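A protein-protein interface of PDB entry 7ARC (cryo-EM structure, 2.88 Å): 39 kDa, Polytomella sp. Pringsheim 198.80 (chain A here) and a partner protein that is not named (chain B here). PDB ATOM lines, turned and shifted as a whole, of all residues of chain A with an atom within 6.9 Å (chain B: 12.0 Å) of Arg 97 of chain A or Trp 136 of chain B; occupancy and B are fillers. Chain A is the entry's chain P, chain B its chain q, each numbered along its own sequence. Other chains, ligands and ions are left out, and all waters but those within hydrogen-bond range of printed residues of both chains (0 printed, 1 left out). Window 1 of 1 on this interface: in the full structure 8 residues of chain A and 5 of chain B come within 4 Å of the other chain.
Hydrophobic or aromatic side chains of chain A that line the printed part of chain B: Val 55, Val 78 and Leu 80.
Hydrophobic or aromatic side chains of chain B that line the printed part of chain A: Trp 136 and Phe 137.
Among the printed residues, 13 pairs touch across the chains.
Among the printed residues, no Asp or Glu carboxylate lies within 4 Å of a Lys or Arg side-chain nitrogen of the other chain.
Of chain B, only Trp 136 (3.2 Å), Asn 138 (2.5 Å), Pro 139 (3.3 Å) and Lys 141 (3.4 Å) come within 4 Å of Arg 97 of chain A.
No residue of chain B comes within 4 Å of Val 29 of chain A.
Gly 75 of chain A touches none of the printed residues of chain B.
Of the printed residues of chain B, Val 78 of chain A touches Trp 136 (3.6 Å) and Phe 137 (3.7 Å).
Arg 93 of chain A touches one residue of chain B.
Ala 94 of chain A touches one residue of chain B.
No residue of chain B comes within 4 Å of Ile 95 of chain A.
Ser 96 of chain A touches just one residue of chain B: Trp 136.
No residue of chain B comes within 4 Å of Ser 98 of chain A.
Of the printed residues of chain A, Pro 139 of chain B touches Arg 97 (3.3 Å).
Of the printed residues of chain A, Asn 138 of chain B touches Arg 97.
Of the printed residues of chain A, Lys 141 of chain B touches Arg 97.
Of the printed residues of chain B, Leu 80 of chain A touches Trp 136 and Phe 137.
Printed residues of chain A within 4 Å of Phe 137 of chain B: Val 78 (3.7 Å) and Leu 80 (3.98 Å).
Arg 142 of chain B touches none of the printed residues of chain A.
The nearest residue of chain A that does not touch Trp 136 of chain B is Val 29 of chain A (4.7 Å).
Among the printed residues, pairs that only touch across the chains: Gln 53 of chain A with Trp 136 of chain B, Val 55 of chain A with Trp 136 of chain B, Val 78 of chain A with Trp 136 of chain B, Val 78 of chain A with Phe 137 of chain B, Leu 80 of chain A with Trp 136 of chain B, Leu 80 of chain A with Phe 137 of chain B, Arg 93 of chain A with Trp 136 of chain B, Ala 94 of chain A with Trp 136 of chain B, Ser 96 of chain A with Trp 136 of chain B and Arg 97 of chain A with Lys 141 of chain B.
NE of Arg 97 of chain A lies within hydrogen-bond range of O of Trp 136 of chain B, at 3.2 Å.
O of Pro 139 of chain B sits at hydrogen-bond distance from NH2 of Arg 97 of chain A (3.3 Å).
The backbone carbonyl oxygen (O) of Asn 138 of chain B is in hydrogen-bond range of the guanidinium group (NH2) of Arg 97 of chain A (2.5 Å).
O of Ala 140 of chain B is in hydrogen-bond range of ND2 of Asn 138 of chain B (2.7 Å).
The backbone carbonyl oxygen (O) of Lys 133 of chain B lies within hydrogen-bond range of the side-chain amide nitrogen (ND2) of Asn 138 of chain B, at 3.4 Å.
O of Val 28 of chain A is in hydrogen-bond range of N of Gln 53 of chain A (3.1 Å).
The side-chain hydroxyl (OG) of Ser 135 of chain B sits close to the backbone NH (N) of Phe 137 of chain B, at 3.3 Å.
The backbone NH (N) of Ala 30 of chain A lies within hydrogen-bond range of the backbone carbonyl oxygen (O) of Gln 53 of chain A.
The side-chain amide nitrogen (NE2) of Gln 53 of chain A lies within hydrogen-bond range of the backbone carbonyl oxygen (O) of Gly 75 of chain A (2.7 Å).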
ATOM      1  N   VAL A  28      16.272  17.711  -9.021  1.00  0.00           N
ATOM      2  CA  VAL A  28      16.261  16.449  -8.296  1.00  0.00           C
ATOM      3  C   VAL A  28      17.695  16.069  -7.964  1.00  0.00           C
ATOM      4  O   VAL A  28      18.514  15.860  -8.865  1.00  0.00           O
ATOM      5  CB  VAL A  28      15.575  15.339  -9.108  1.00  0.00           C
ATOM      6  CG1 VAL A  28      15.755  14.000  -8.434  1.00  0.00           C
ATOM      7  CG2 VAL A  28      14.102  15.653  -9.287  1.00  0.00           C
ATOM      8  N   VAL A  29      18.001  15.989  -6.674  1.00  0.00           N
ATOM      9  CA  VAL A  29      19.238  15.394  -6.183  1.00  0.00           C
ATOM     10  C   VAL A  29      18.867  14.066  -5.541  1.00  0.00           C
ATOM     11  O   VAL A  29      18.046  14.026  -4.618  1.00  0.00           O
ATOM     12  CB  VAL A  29      19.961  16.316  -5.192  1.00  0.00           C
ATOM     13  CG1 VAL A  29      21.276  15.699  -4.761  1.00  0.00           C
ATOM     14  CG2 VAL A  29      20.196  17.673  -5.819  1.00  0.00           C
ATOM     15  N   ALA A  30      19.459  12.980  -6.029  1.00  0.00           N
ATOM     16  CA  ALA A  30      19.032  11.637  -5.670  1.00  0.00           C
ATOM     17  C   ALA A  30      20.190  10.852  -5.073  1.00  0.00           C
ATOM     18  O   ALA A  30      21.312  10.899  -5.583  1.00  0.00           O
ATOM     19  CB  ALA A  30      18.481  10.893  -6.888  1.00  0.00           C
ATOM     20  N   THR A  31      19.909  10.135  -3.990  1.00  0.00           N
ATOM     21  CA  THR A  31      20.834   9.168  -3.408  1.00  0.00           C
ATOM     22  C   THR A  31      20.289   7.773  -3.687  1.00  0.00           C
ATOM     23  O   THR A  31      19.362   7.317  -3.015  1.00  0.00           O
ATOM     24  CB  THR A  31      21.016   9.394  -1.913  1.00  0.00           C
ATOM     25  OG1 THR A  31      21.372  10.758  -1.676  1.00  0.00           O
ATOM     26  CG2 THR A  31      22.112   8.499  -1.377  1.00  0.00           C
ATOM     27  N   GLN A  53      21.091  15.460 -10.543  1.00  0.00           N
ATOM     28  CA  GLN A  53      22.317  15.043  -9.878  1.00  0.00           C
ATOM     29  C   GLN A  53      22.040  13.809  -9.029  1.00  0.00           C
ATOM     30  O   GLN A  53      21.095  13.799  -8.235  1.00  0.00           O
ATOM     31  CB  GLN A  53      22.880  16.175  -9.019  1.00  0.00           C
ATOM     32  CG  GLN A  53      24.000  15.753  -8.095  1.00  0.00           C
ATOM     33  CD  GLN A  53      24.751  16.935  -7.535  1.00  0.00           C
ATOM     34  OE1 GLN A  53      24.181  17.779  -6.849  1.00  0.00           O
ATOM     35  NE2 GLN A  53      26.040  17.009  -7.833  1.00  0.00           N
ATOM     36  N   VAL A  55      23.653  10.969  -6.392  1.00  0.00           N
ATOM     37  CA  VAL A  55      24.702  10.527  -5.479  1.00  0.00           C
ATOM     38  C   VAL A  55      24.633   9.009  -5.380  1.00  0.00           C
ATOM     39  O   VAL A  55      23.591   8.451  -5.022  1.00  0.00           O
ATOM     40  CB  VAL A  55      24.548  11.178  -4.098  1.00  0.00           C
ATOM     41  CG1 VAL A  55      25.744  10.857  -3.227  1.00  0.00           C
ATOM     42  CG2 VAL A  55      24.384  12.676  -4.244  1.00  0.00           C
ATOM     43  N   GLY A  75      29.946  16.709 -12.721  1.00  0.00           N
ATOM     44  CA  GLY A  75      29.476  16.948 -11.377  1.00  0.00           C
ATOM     45  C   GLY A  75      28.094  16.419 -11.068  1.00  0.00           C
ATOM     46  O   GLY A  75      27.593  16.657  -9.962  1.00  0.00           O
ATOM     47  N   VAL A  78      27.751  11.648  -8.541  1.00  0.00           N
ATOM     48  CA  VAL A  78      28.699  11.701  -7.434  1.00  0.00           C
ATOM     49  C   VAL A  78      28.862  10.296  -6.871  1.00  0.00           C
ATOM     50  O   VAL A  78      27.891   9.689  -6.404  1.00  0.00           O
ATOM     51  CB  VAL A  78      28.231  12.679  -6.347  1.00  0.00           C
ATOM     52  CG1 VAL A  78      29.096  12.546  -5.108  1.00  0.00           C
ATOM     53  CG2 VAL A  78      28.257  14.095  -6.873  1.00  0.00           C
ATOM     54  N   LEU A  80      30.452   7.985  -4.094  1.00  0.00           N
ATOM     55  CA  LEU A  80      31.032   7.982  -2.754  1.00  0.00           C
ATOM     56  C   LEU A  80      31.753   6.665  -2.480  1.00  0.00           C
ATOM     57  O   LEU A  80      31.147   5.597  -2.608  1.00  0.00           O
ATOM     58  CB  LEU A  80      29.965   8.223  -1.704  1.00  0.00           C
ATOM     59  CG  LEU A  80      29.298   9.594  -1.721  1.00  0.00           C
ATOM     60  CD1 LEU A  80      28.172   9.633  -0.710  1.00  0.00           C
ATOM     61  CD2 LEU A  80      30.314  10.679  -1.442  1.00  0.00           C
ATOM     62  N   ARG A  92      23.986   9.578   6.660  1.00  0.00           N
ATOM     63  CA  ARG A  92      23.565  10.969   6.793  1.00  0.00           C
ATOM     64  C   ARG A  92      24.312  11.862   5.814  1.00  0.00           C
ATOM     65  O   ARG A  92      23.721  12.766   5.212  1.00  0.00           O
ATOM     66  CB  ARG A  92      23.763  11.467   8.224  1.00  0.00           C
ATOM     67  CG  ARG A  92      22.855  10.822   9.248  1.00  0.00           C
ATOM     68  CD  ARG A  92      23.110  11.387  10.634  1.00  0.00           C
ATOM     69  NE  ARG A  92      22.232  10.793  11.634  1.00  0.00           N
ATOM     70  CZ  ARG A  92      22.530   9.715  12.346  1.00  0.00           C
ATOM     71  NH1 ARG A  92      23.722   9.146  12.269  1.00  0.00           N
ATOM     72  NH2 ARG A  92      21.622   9.214  13.175  1.00  0.00           N
ATOM     73  N   ARG A  93      25.616  11.633   5.646  1.00  0.00           N
ATOM     74  CA  ARG A  93      26.383  12.429   4.694  1.00  0.00           C
ATOM     75  C   ARG A  93      25.891  12.211   3.269  1.00  0.00           C
ATOM     76  O   ARG A  93      25.841  13.155   2.472  1.00  0.00           O
ATOM     77  CB  ARG A  93      27.869  12.089   4.803  1.00  0.00           C
ATOM     78  CG  ARG A  93      28.733  12.763   3.753  1.00  0.00           C
ATOM     79  CD  ARG A  93      29.868  11.864   3.301  1.00  0.00           C
ATOM     80  NE  ARG A  93      30.858  12.593   2.517  1.00  0.00           N
ATOM     81  CZ  ARG A  93      31.910  12.036   1.934  1.00  0.00           C
ATOM     82  NH1 ARG A  93      32.145  10.737   2.028  1.00  0.00           N
ATOM     83  NH2 ARG A  93      32.748  12.800   1.242  1.00  0.00           N
ATOM     84  N   ALA A  94      25.527  10.975   2.929  1.00  0.00           N
ATOM     85  CA  ALA A  94      25.121  10.664   1.561  1.00  0.00           C
ATOM     86  C   ALA A  94      23.830  11.378   1.182  1.00  0.00           C
ATOM     87  O   ALA A  94      23.699  11.872   0.056  1.00  0.00           O
ATOM     88  CB  ALA A  94      24.970   9.155   1.391  1.00  0.00           C
ATOM     89  N   ILE A  95      22.869  11.447   2.096  1.00  0.00           N
ATOM     90  CA  ILE A  95      21.570  12.039   1.808  1.00  0.00           C
ATOM     91  C   ILE A  95      21.508  13.498   2.260  1.00  0.00           C
ATOM     92  O   ILE A  95      20.420  14.049   2.412  1.00  0.00           O
ATOM     93  CB  ILE A  95      20.421  11.227   2.421  1.00  0.00           C
ATOM     94  CG1 ILE A  95      20.530  11.202   3.940  1.00  0.00           C
ATOM     95  CG2 ILE A  95      20.433   9.809   1.892  1.00  0.00           C
ATOM     96  CD1 ILE A  95      19.314  10.629   4.605  1.00  0.00           C
ATOM     97  N   SER A  96      22.662  14.126   2.497  1.00  0.00           N
ATOM     98  CA  SER A  96      22.679  15.487   3.021  1.00  0.00           C
ATOM     99  C   SER A  96      21.966  16.451   2.082  1.00  0.00           C
ATOM    100  O   SER A  96      21.101  17.224   2.507  1.00  0.00           O
ATOM    101  CB  SER A  96      24.120  15.931   3.267  1.00  0.00           C
ATOM    102  OG  SER A  96      24.859  15.958   2.060  1.00  0.00           O
ATOM    103  N   ARG A  97      22.317  16.424   0.799  1.00  0.00           N
ATOM    104  CA  ARG A  97      21.755  17.348  -0.175  1.00  0.00           C
ATOM    105  C   ARG A  97      20.604  16.745  -0.969  1.00  0.00           C
ATOM    106  O   ARG A  97      20.048  17.422  -1.837  1.00  0.00           O
ATOM    107  CB  ARG A  97      22.838  17.820  -1.148  1.00  0.00           C
ATOM    108  CG  ARG A  97      24.100  18.346  -0.497  1.00  0.00           C
ATOM    109  CD  ARG A  97      24.922  19.125  -1.506  1.00  0.00           C
ATOM    110  NE  ARG A  97      26.237  19.483  -0.995  1.00  0.00           N
ATOM    111  CZ  ARG A  97      26.548  20.676  -0.508  1.00  0.00           C
ATOM    112  NH1 ARG A  97      25.658  21.652  -0.450  1.00  0.00           N
ATOM    113  NH2 ARG A  97      27.784  20.896  -0.070  1.00  0.00           N
ATOM    114  N   SER A  98      20.230  15.501  -0.689  1.00  0.00           N
ATOM    115  CA  SER A  98      19.291  14.770  -1.527  1.00  0.00           C
ATOM    116  C   SER A  98      17.853  15.014  -1.096  1.00  0.00           C
ATOM    117  O   SER A  98      17.532  14.990   0.095  1.00  0.00           O
ATOM    118  CB  SER A  98      19.591  13.275  -1.488  1.00  0.00           C
ATOM    119  OG  SER A  98      20.946  13.030  -1.812  1.00  0.00           O
ATOM    120  N   ASN A  99      16.994  15.253  -2.081  1.00  0.00           N
ATOM    121  CA  ASN A  99      15.564  15.405  -1.867  1.00  0.00           C
ATOM    122  C   ASN A  99      14.746  14.187  -2.289  1.00  0.00           C
ATOM    123  O   ASN A  99      13.534  14.171  -2.057  1.00  0.00           O
ATOM    124  CB  ASN A  99      15.073  16.676  -2.575  1.00  0.00           C
ATOM    125  CG  ASN A  99      15.257  16.625  -4.079  1.00  0.00           C
ATOM    126  OD1 ASN A  99      15.637  15.602  -4.643  1.00  0.00           O
ATOM    127  ND2 ASN A  99      15.019  17.753  -4.734  1.00  0.00           N
ATOM    128  N   VAL A 100      15.370  13.178  -2.897  1.00  0.00           N
ATOM    129  CA  VAL A 100      14.737  11.888  -3.166  1.00  0.00           C
ATOM    130  C   VAL A 100      15.760  10.796  -2.879  1.00  0.00           C
ATOM    131  O   VAL A 100      16.946  10.946  -3.188  1.00  0.00           O
ATOM    132  CB  VAL A 100      14.205  11.767  -4.613  1.00  0.00           C
ATOM    133  CG1 VAL A 100      13.137  12.803  -4.893  1.00  0.00           C
ATOM    134  CG2 VAL A 100      15.317  11.887  -5.612  1.00  0.00           C
ATOM    135  N   LYS A 136      14.388  17.095   4.671  1.00  0.00           N
ATOM    136  CA  LYS A 136      14.617  17.603   3.322  1.00  0.00           C
ATOM    137  C   LYS A 136      14.182  16.594   2.266  1.00  0.00           C
ATOM    138  O   LYS A 136      13.657  16.977   1.214  1.00  0.00           O
ATOM    139  CB  LYS A 136      16.090  17.974   3.143  1.00  0.00           C
ATOM    140  CG  LYS A 136      16.446  18.433   1.738  1.00  0.00           C
ATOM    141  CD  LYS A 136      17.951  18.547   1.546  1.00  0.00           C
ATOM    142  CE  LYS A 136      18.585  19.413   2.623  1.00  0.00           C
ATOM    143  NZ  LYS A 136      19.601  20.346   2.063  1.00  0.00           N
ATOM    144  N   VAL A 137      14.397  15.305   2.524  1.00  0.00           N
ATOM    145  CA  VAL A 137      13.988  14.266   1.585  1.00  0.00           C
ATOM    146  C   VAL A 137      12.475  14.285   1.444  1.00  0.00           C
ATOM    147  O   VAL A 137      11.740  14.182   2.434  1.00  0.00           O
ATOM    148  CB  VAL A 137      14.490  12.896   2.045  1.00  0.00           C
ATOM    149  CG1 VAL A 137      14.206  11.849   0.985  1.00  0.00           C
ATOM    150  CG2 VAL A 137      15.974  12.956   2.357  1.00  0.00           C
ATOM    151  N   GLU B 128      41.506  13.814  -4.051  1.00  0.00           N
ATOM    152  CA  GLU B 128      40.195  14.412  -3.833  1.00  0.00           C
ATOM    153  C   GLU B 128      40.383  15.736  -3.088  1.00  0.00           C
ATOM    154  O   GLU B 128      39.823  15.959  -2.013  1.00  0.00           O
ATOM    155  CB  GLU B 128      39.283  13.443  -3.063  1.00  0.00           C
ATOM    156  CG  GLU B 128      37.854  13.931  -2.827  1.00  0.00           C
ATOM    157  CD  GLU B 128      37.067  14.092  -4.112  1.00  0.00           C
ATOM    158  OE1 GLU B 128      37.390  13.406  -5.103  1.00  0.00           O
ATOM    159  OE2 GLU B 128      36.129  14.916  -4.132  1.00  0.00           O
ATOM    160  N   CYS B 129      41.222  16.605  -3.651  1.00  0.00           N
ATOM    161  CA  CYS B 129      41.534  17.889  -3.036  1.00  0.00           C
ATOM    162  C   CYS B 129      40.850  19.062  -3.728  1.00  0.00           C
ATOM    163  O   CYS B 129      40.173  19.857  -3.072  1.00  0.00           O
ATOM    164  CB  CYS B 129      43.051  18.108  -3.016  1.00  0.00           C
ATOM    165  SG  CYS B 129      43.923  17.167  -1.741  1.00  0.00           S
ATOM    166  N   TYR B 130      41.006  19.184  -5.045  1.00  0.00           N
ATOM    167  CA  TYR B 130      40.439  20.296  -5.800  1.00  0.00           C
ATOM    168  C   TYR B 130      39.173  19.879  -6.532  1.00  0.00           C
ATOM    169  O   TYR B 130      39.177  18.900  -7.284  1.00  0.00           O
ATOM    170  CB  TYR B 130      41.444  20.849  -6.810  1.00  0.00           C
ATOM    171  CG  TYR B 130      40.819  21.861  -7.741  1.00  0.00           C
ATOM    172  CD1 TYR B 130      40.370  23.084  -7.269  1.00  0.00           C
ATOM    173  CD2 TYR B 130      40.647  21.576  -9.087  1.00  0.00           C
ATOM    174  CE1 TYR B 130      39.787  24.001  -8.115  1.00  0.00           C
ATOM    175  CE2 TYR B 130      40.063  22.486  -9.939  1.00  0.00           C
ATOM    176  CZ  TYR B 130      39.636  23.696  -9.448  1.00  0.00           C
ATOM    177  OH  TYR B 130      39.052  24.606 -10.297  1.00  0.00           O
ATOM    178  N   ASN B 131      38.100  20.625  -6.312  1.00  0.00           N
ATOM    179  CA  ASN B 131      36.863  20.498  -7.061  1.00  0.00           C
ATOM    180  C   ASN B 131      36.303  21.890  -7.306  1.00  0.00           C
ATOM    181  O   ASN B 131      36.613  22.828  -6.562  1.00  0.00           O
ATOM    182  CB  ASN B 131      35.832  19.640  -6.316  1.00  0.00           C
ATOM    183  CG  ASN B 131      36.285  18.206  -6.138  1.00  0.00           C
ATOM    184  OD1 ASN B 131      36.510  17.745  -5.019  1.00  0.00           O
ATOM    185  ND2 ASN B 131      36.411  17.489  -7.248  1.00  0.00           N
ATOM    186  N   PRO B 132      35.491  22.060  -8.347  1.00  0.00           N
ATOM    187  CA  PRO B 132      34.847  23.357  -8.580  1.00  0.00           C
ATOM    188  C   PRO B 132      33.900  23.721  -7.446  1.00  0.00           C
ATOM    189  O   PRO B 132      33.466  22.876  -6.663  1.00  0.00           O
ATOM    190  CB  PRO B 132      34.093  23.143  -9.897  1.00  0.00           C
ATOM    191  CG  PRO B 132      34.856  22.042 -10.562  1.00  0.00           C
ATOM    192  CD  PRO B 132      35.188  21.119  -9.434  1.00  0.00           C
ATOM    193  N   LYS B 133      33.594  25.016  -7.354  1.00  0.00           N
ATOM    194  CA  LYS B 133      32.770  25.504  -6.255  1.00  0.00           C
ATOM    195  C   LYS B 133      31.315  25.075  -6.383  1.00  0.00           C
ATOM    196  O   LYS B 133      30.578  25.129  -5.394  1.00  0.00           O
ATOM    197  CB  LYS B 133      32.865  27.025  -6.170  1.00  0.00           C
ATOM    198  CG  LYS B 133      34.278  27.528  -5.958  1.00  0.00           C
ATOM    199  CD  LYS B 133      34.390  29.013  -6.228  1.00  0.00           C
ATOM    200  CE  LYS B 133      35.241  29.686  -5.175  1.00  0.00           C
ATOM    201  NZ  LYS B 133      36.516  28.954  -4.961  1.00  0.00           N
ATOM    202  N   GLY B 134      30.887  24.653  -7.565  1.00  0.00           N
ATOM    203  CA  GLY B 134      29.563  24.108  -7.757  1.00  0.00           C
ATOM    204  C   GLY B 134      29.450  22.628  -7.493  1.00  0.00           C
ATOM    205  O   GLY B 134      28.385  22.043  -7.711  1.00  0.00           O
ATOM    206  N   SER B 135      30.524  22.000  -7.022  1.00  0.00           N
ATOM    207  CA  SER B 135      30.538  20.563  -6.804  1.00  0.00           C
ATOM    208  C   SER B 135      29.744  20.181  -5.561  1.00  0.00           C
ATOM    209  O   SER B 135      29.593  20.967  -4.624  1.00  0.00           O
ATOM    210  CB  SER B 135      31.976  20.063  -6.671  1.00  0.00           C
ATOM    211  OG  SER B 135      32.012  18.670  -6.426  1.00  0.00           O
ATOM    212  N   TRP B 136      29.231  18.949  -5.572  1.00  0.00           N
ATOM    213  CA  TRP B 136      28.548  18.400  -4.405  1.00  0.00           C
ATOM    214  C   TRP B 136      29.475  18.327  -3.200  1.00  0.00           C
ATOM    215  O   TRP B 136      29.027  18.471  -2.058  1.00  0.00           O
ATOM    216  CB  TRP B 136      28.003  17.013  -4.751  1.00  0.00           C
ATOM    217  CG  TRP B 136      27.150  16.369  -3.708  1.00  0.00           C
ATOM    218  CD1 TRP B 136      25.798  16.463  -3.592  1.00  0.00           C
ATOM    219  CD2 TRP B 136      27.586  15.504  -2.653  1.00  0.00           C
ATOM    220  NE1 TRP B 136      25.362  15.723  -2.522  1.00  0.00           N
ATOM    221  CE2 TRP B 136      26.441  15.124  -1.928  1.00  0.00           C
ATOM    222  CE3 TRP B 136      28.831  15.022  -2.245  1.00  0.00           C
ATOM    223  CZ2 TRP B 136      26.504  14.285  -0.820  1.00  0.00           C
ATOM    224  CZ3 TRP B 136      28.891  14.189  -1.146  1.00  0.00           C
ATOM    225  CH2 TRP B 136      27.736  13.829  -0.446  1.00  0.00           C
ATOM    226  N   PHE B 137      30.767  18.105  -3.438  1.00  0.00           N
ATOM    227  CA  PHE B 137      31.733  17.976  -2.354  1.00  0.00           C
ATOM    228  C   PHE B 137      31.998  19.304  -1.658  1.00  0.00           C
ATOM    229  O   PHE B 137      32.385  19.317  -0.485  1.00  0.00           O
ATOM    230  CB  PHE B 137      33.032  17.381  -2.888  1.00  0.00           C
ATOM    231  CG  PHE B 137      32.884  15.979  -3.393  1.00  0.00           C
ATOM    232  CD1 PHE B 137      32.623  14.941  -2.517  1.00  0.00           C
ATOM    233  CD2 PHE B 137      32.983  15.701  -4.743  1.00  0.00           C
ATOM    234  CE1 PHE B 137      32.480  13.650  -2.976  1.00  0.00           C
ATOM    235  CE2 PHE B 137      32.838  14.413  -5.209  1.00  0.00           C
ATOM    236  CZ  PHE B 137      32.586  13.386  -4.326  1.00  0.00           C
ATOM    237  N   ASN B 138      31.820  20.416  -2.361  1.00  0.00           N
ATOM    238  CA  ASN B 138      32.148  21.720  -1.804  1.00  0.00           C
ATOM    239  C   ASN B 138      31.309  21.996  -0.561  1.00  0.00           C
ATOM    240  O   ASN B 138      30.086  21.800  -0.588  1.00  0.00           O
ATOM    241  CB  ASN B 138      31.911  22.813  -2.843  1.00  0.00           C
ATOM    242  CG  ASN B 138      32.715  24.062  -2.564  1.00  0.00           C
ATOM    243  OD1 ASN B 138      33.942  24.030  -2.553  1.00  0.00           O
ATOM    244  ND2 ASN B 138      32.024  25.170  -2.333  1.00  0.00           N
ATOM    245  N   PRO B 139      31.927  22.423   0.552  1.00  0.00           N
ATOM    246  CA  PRO B 139      31.164  22.740   1.768  1.00  0.00           C
ATOM    247  C   PRO B 139      29.994  23.681   1.527  1.00  0.00           C
ATOM    248  O   PRO B 139      28.850  23.354   1.851  1.00  0.00           O
ATOM    249  CB  PRO B 139      32.222  23.392   2.662  1.00  0.00           C
ATOM    250  CG  PRO B 139      33.466  22.662   2.298  1.00  0.00           C
ATOM    251  CD  PRO B 139      33.379  22.461   0.799  1.00  0.00           C
ATOM    252  N   ALA B 140      30.270  24.853   0.958  1.00  0.00           N
ATOM    253  CA  ALA B 140      29.230  25.807   0.582  1.00  0.00           C
ATOM    254  C   ALA B 140      29.053  25.726  -0.931  1.00  0.00           C
ATOM    255  O   ALA B 140      29.689  26.459  -1.689  1.00  0.00           O
ATOM    256  CB  ALA B 140      29.592  27.214   1.036  1.00  0.00           C
ATOM    257  N   LYS B 141      28.179  24.824  -1.364  1.00  0.00           N
ATOM    258  CA  LYS B 141      27.918  24.649  -2.786  1.00  0.00           C
ATOM    259  C   LYS B 141      27.268  25.898  -3.364  1.00  0.00           C
ATOM    260  O   LYS B 141      26.471  26.567  -2.702  1.00  0.00           O
ATOM    261  CB  LYS B 141      27.023  23.433  -3.012  1.00  0.00           C
ATOM    262  CG  LYS B 141      27.023  22.914  -4.433  1.00  0.00           C
ATOM    263  CD  LYS B 141      26.070  21.746  -4.592  1.00  0.00           C
ATOM    264  CE  LYS B 141      25.416  21.756  -5.962  1.00  0.00           C
ATOM    265  NZ  LYS B 141      24.328  22.767  -6.058  1.00  0.00           N
ATOM    266  N   ARG B 142      27.616  26.216  -4.606  1.00  0.00           N
ATOM    267  CA  ARG B 142      27.201  27.456  -5.246  1.00  0.00           C
ATOM    268  C   ARG B 142      26.198  27.152  -6.350  1.00  0.00           C
ATOM    269  O   ARG B 142      26.498  26.379  -7.265  1.00  0.00           O
ATOM    270  CB  ARG B 142      28.403  28.198  -5.828  1.00  0.00           C
ATOM    271  CG  ARG B 142      29.372  28.712  -4.795  1.00  0.00           C
ATOM    272  CD  ARG B 142      30.030  29.990  -5.255  1.00  0.00           C
ATOM    273  NE  ARG B 142      30.991  30.476  -4.272  1.00  0.00           N
ATOM    274  CZ  ARG B 142      31.872  31.439  -4.502  1.00  0.00           C
ATOM    275  NH1 ARG B 142      31.895  32.092  -5.651  1.00  0.00           N
ATOM    276  NH2 ARG B 142      32.742  31.761  -3.551  1.00  0.00           N
ATOM    277  N   ASN B 143      25.012  27.751  -6.260  1.00  0.00           N
ATOM    278  CA  ASN B 143      24.128  27.894  -7.411  1.00  0.00           C
ATOM    279  C   ASN B 143      24.374  29.278  -8.011  1.00  0.00           C
ATOM    280  O   ASN B 143      24.078  30.305  -7.398  1.00  0.00           O
ATOM    281  CB  ASN B 143      22.662  27.609  -7.055  1.00  0.00           C
ATOM    282  CG  ASN B 143      22.053  28.572  -6.024  1.00  0.00           C
ATOM    283  OD1 ASN B 143      20.934  28.414  -5.552  1.00  0.00           O
ATOM    284  ND2 ASN B 143      22.832  29.587  -5.667  1.00  0.00           N
ATOM    285  N   TRP B 144      24.945  29.304  -9.211  1.00  0.00           N
ATOM    286  CA  TRP B 144      25.441  30.553  -9.782  1.00  0.00           C
ATOM    287  C   TRP B 144      24.294  31.362 -10.389  1.00  0.00           C
ATOM    288  O   TRP B 144      24.238  31.638 -11.585  1.00  0.00           O
ATOM    289  CB  TRP B 144      26.529  30.266 -10.806  1.00  0.00           C
ATOM    290  CG  TRP B 144      27.499  29.202 -10.385  1.00  0.00           C
ATOM    291  CD1 TRP B 144      27.280  27.857 -10.352  1.00  0.00           C
ATOM    292  CD2 TRP B 144      28.844  29.398  -9.940  1.00  0.00           C
ATOM    293  NE1 TRP B 144      28.403  27.204  -9.915  1.00  0.00           N
ATOM    294  CE2 TRP B 144      29.378  28.129  -9.655  1.00  0.00           C
ATOM    295  CE3 TRP B 144      29.648  30.524  -9.751  1.00  0.00           C
ATOM    296  CZ2 TRP B 144      30.679  27.955  -9.195  1.00  0.00           C
ATOM    297  CZ3 TRP B 144      30.937  30.348  -9.298  1.00  0.00           C
ATOM    298  CH2 TRP B 144      31.440  29.075  -9.024  1.00  0.00           C
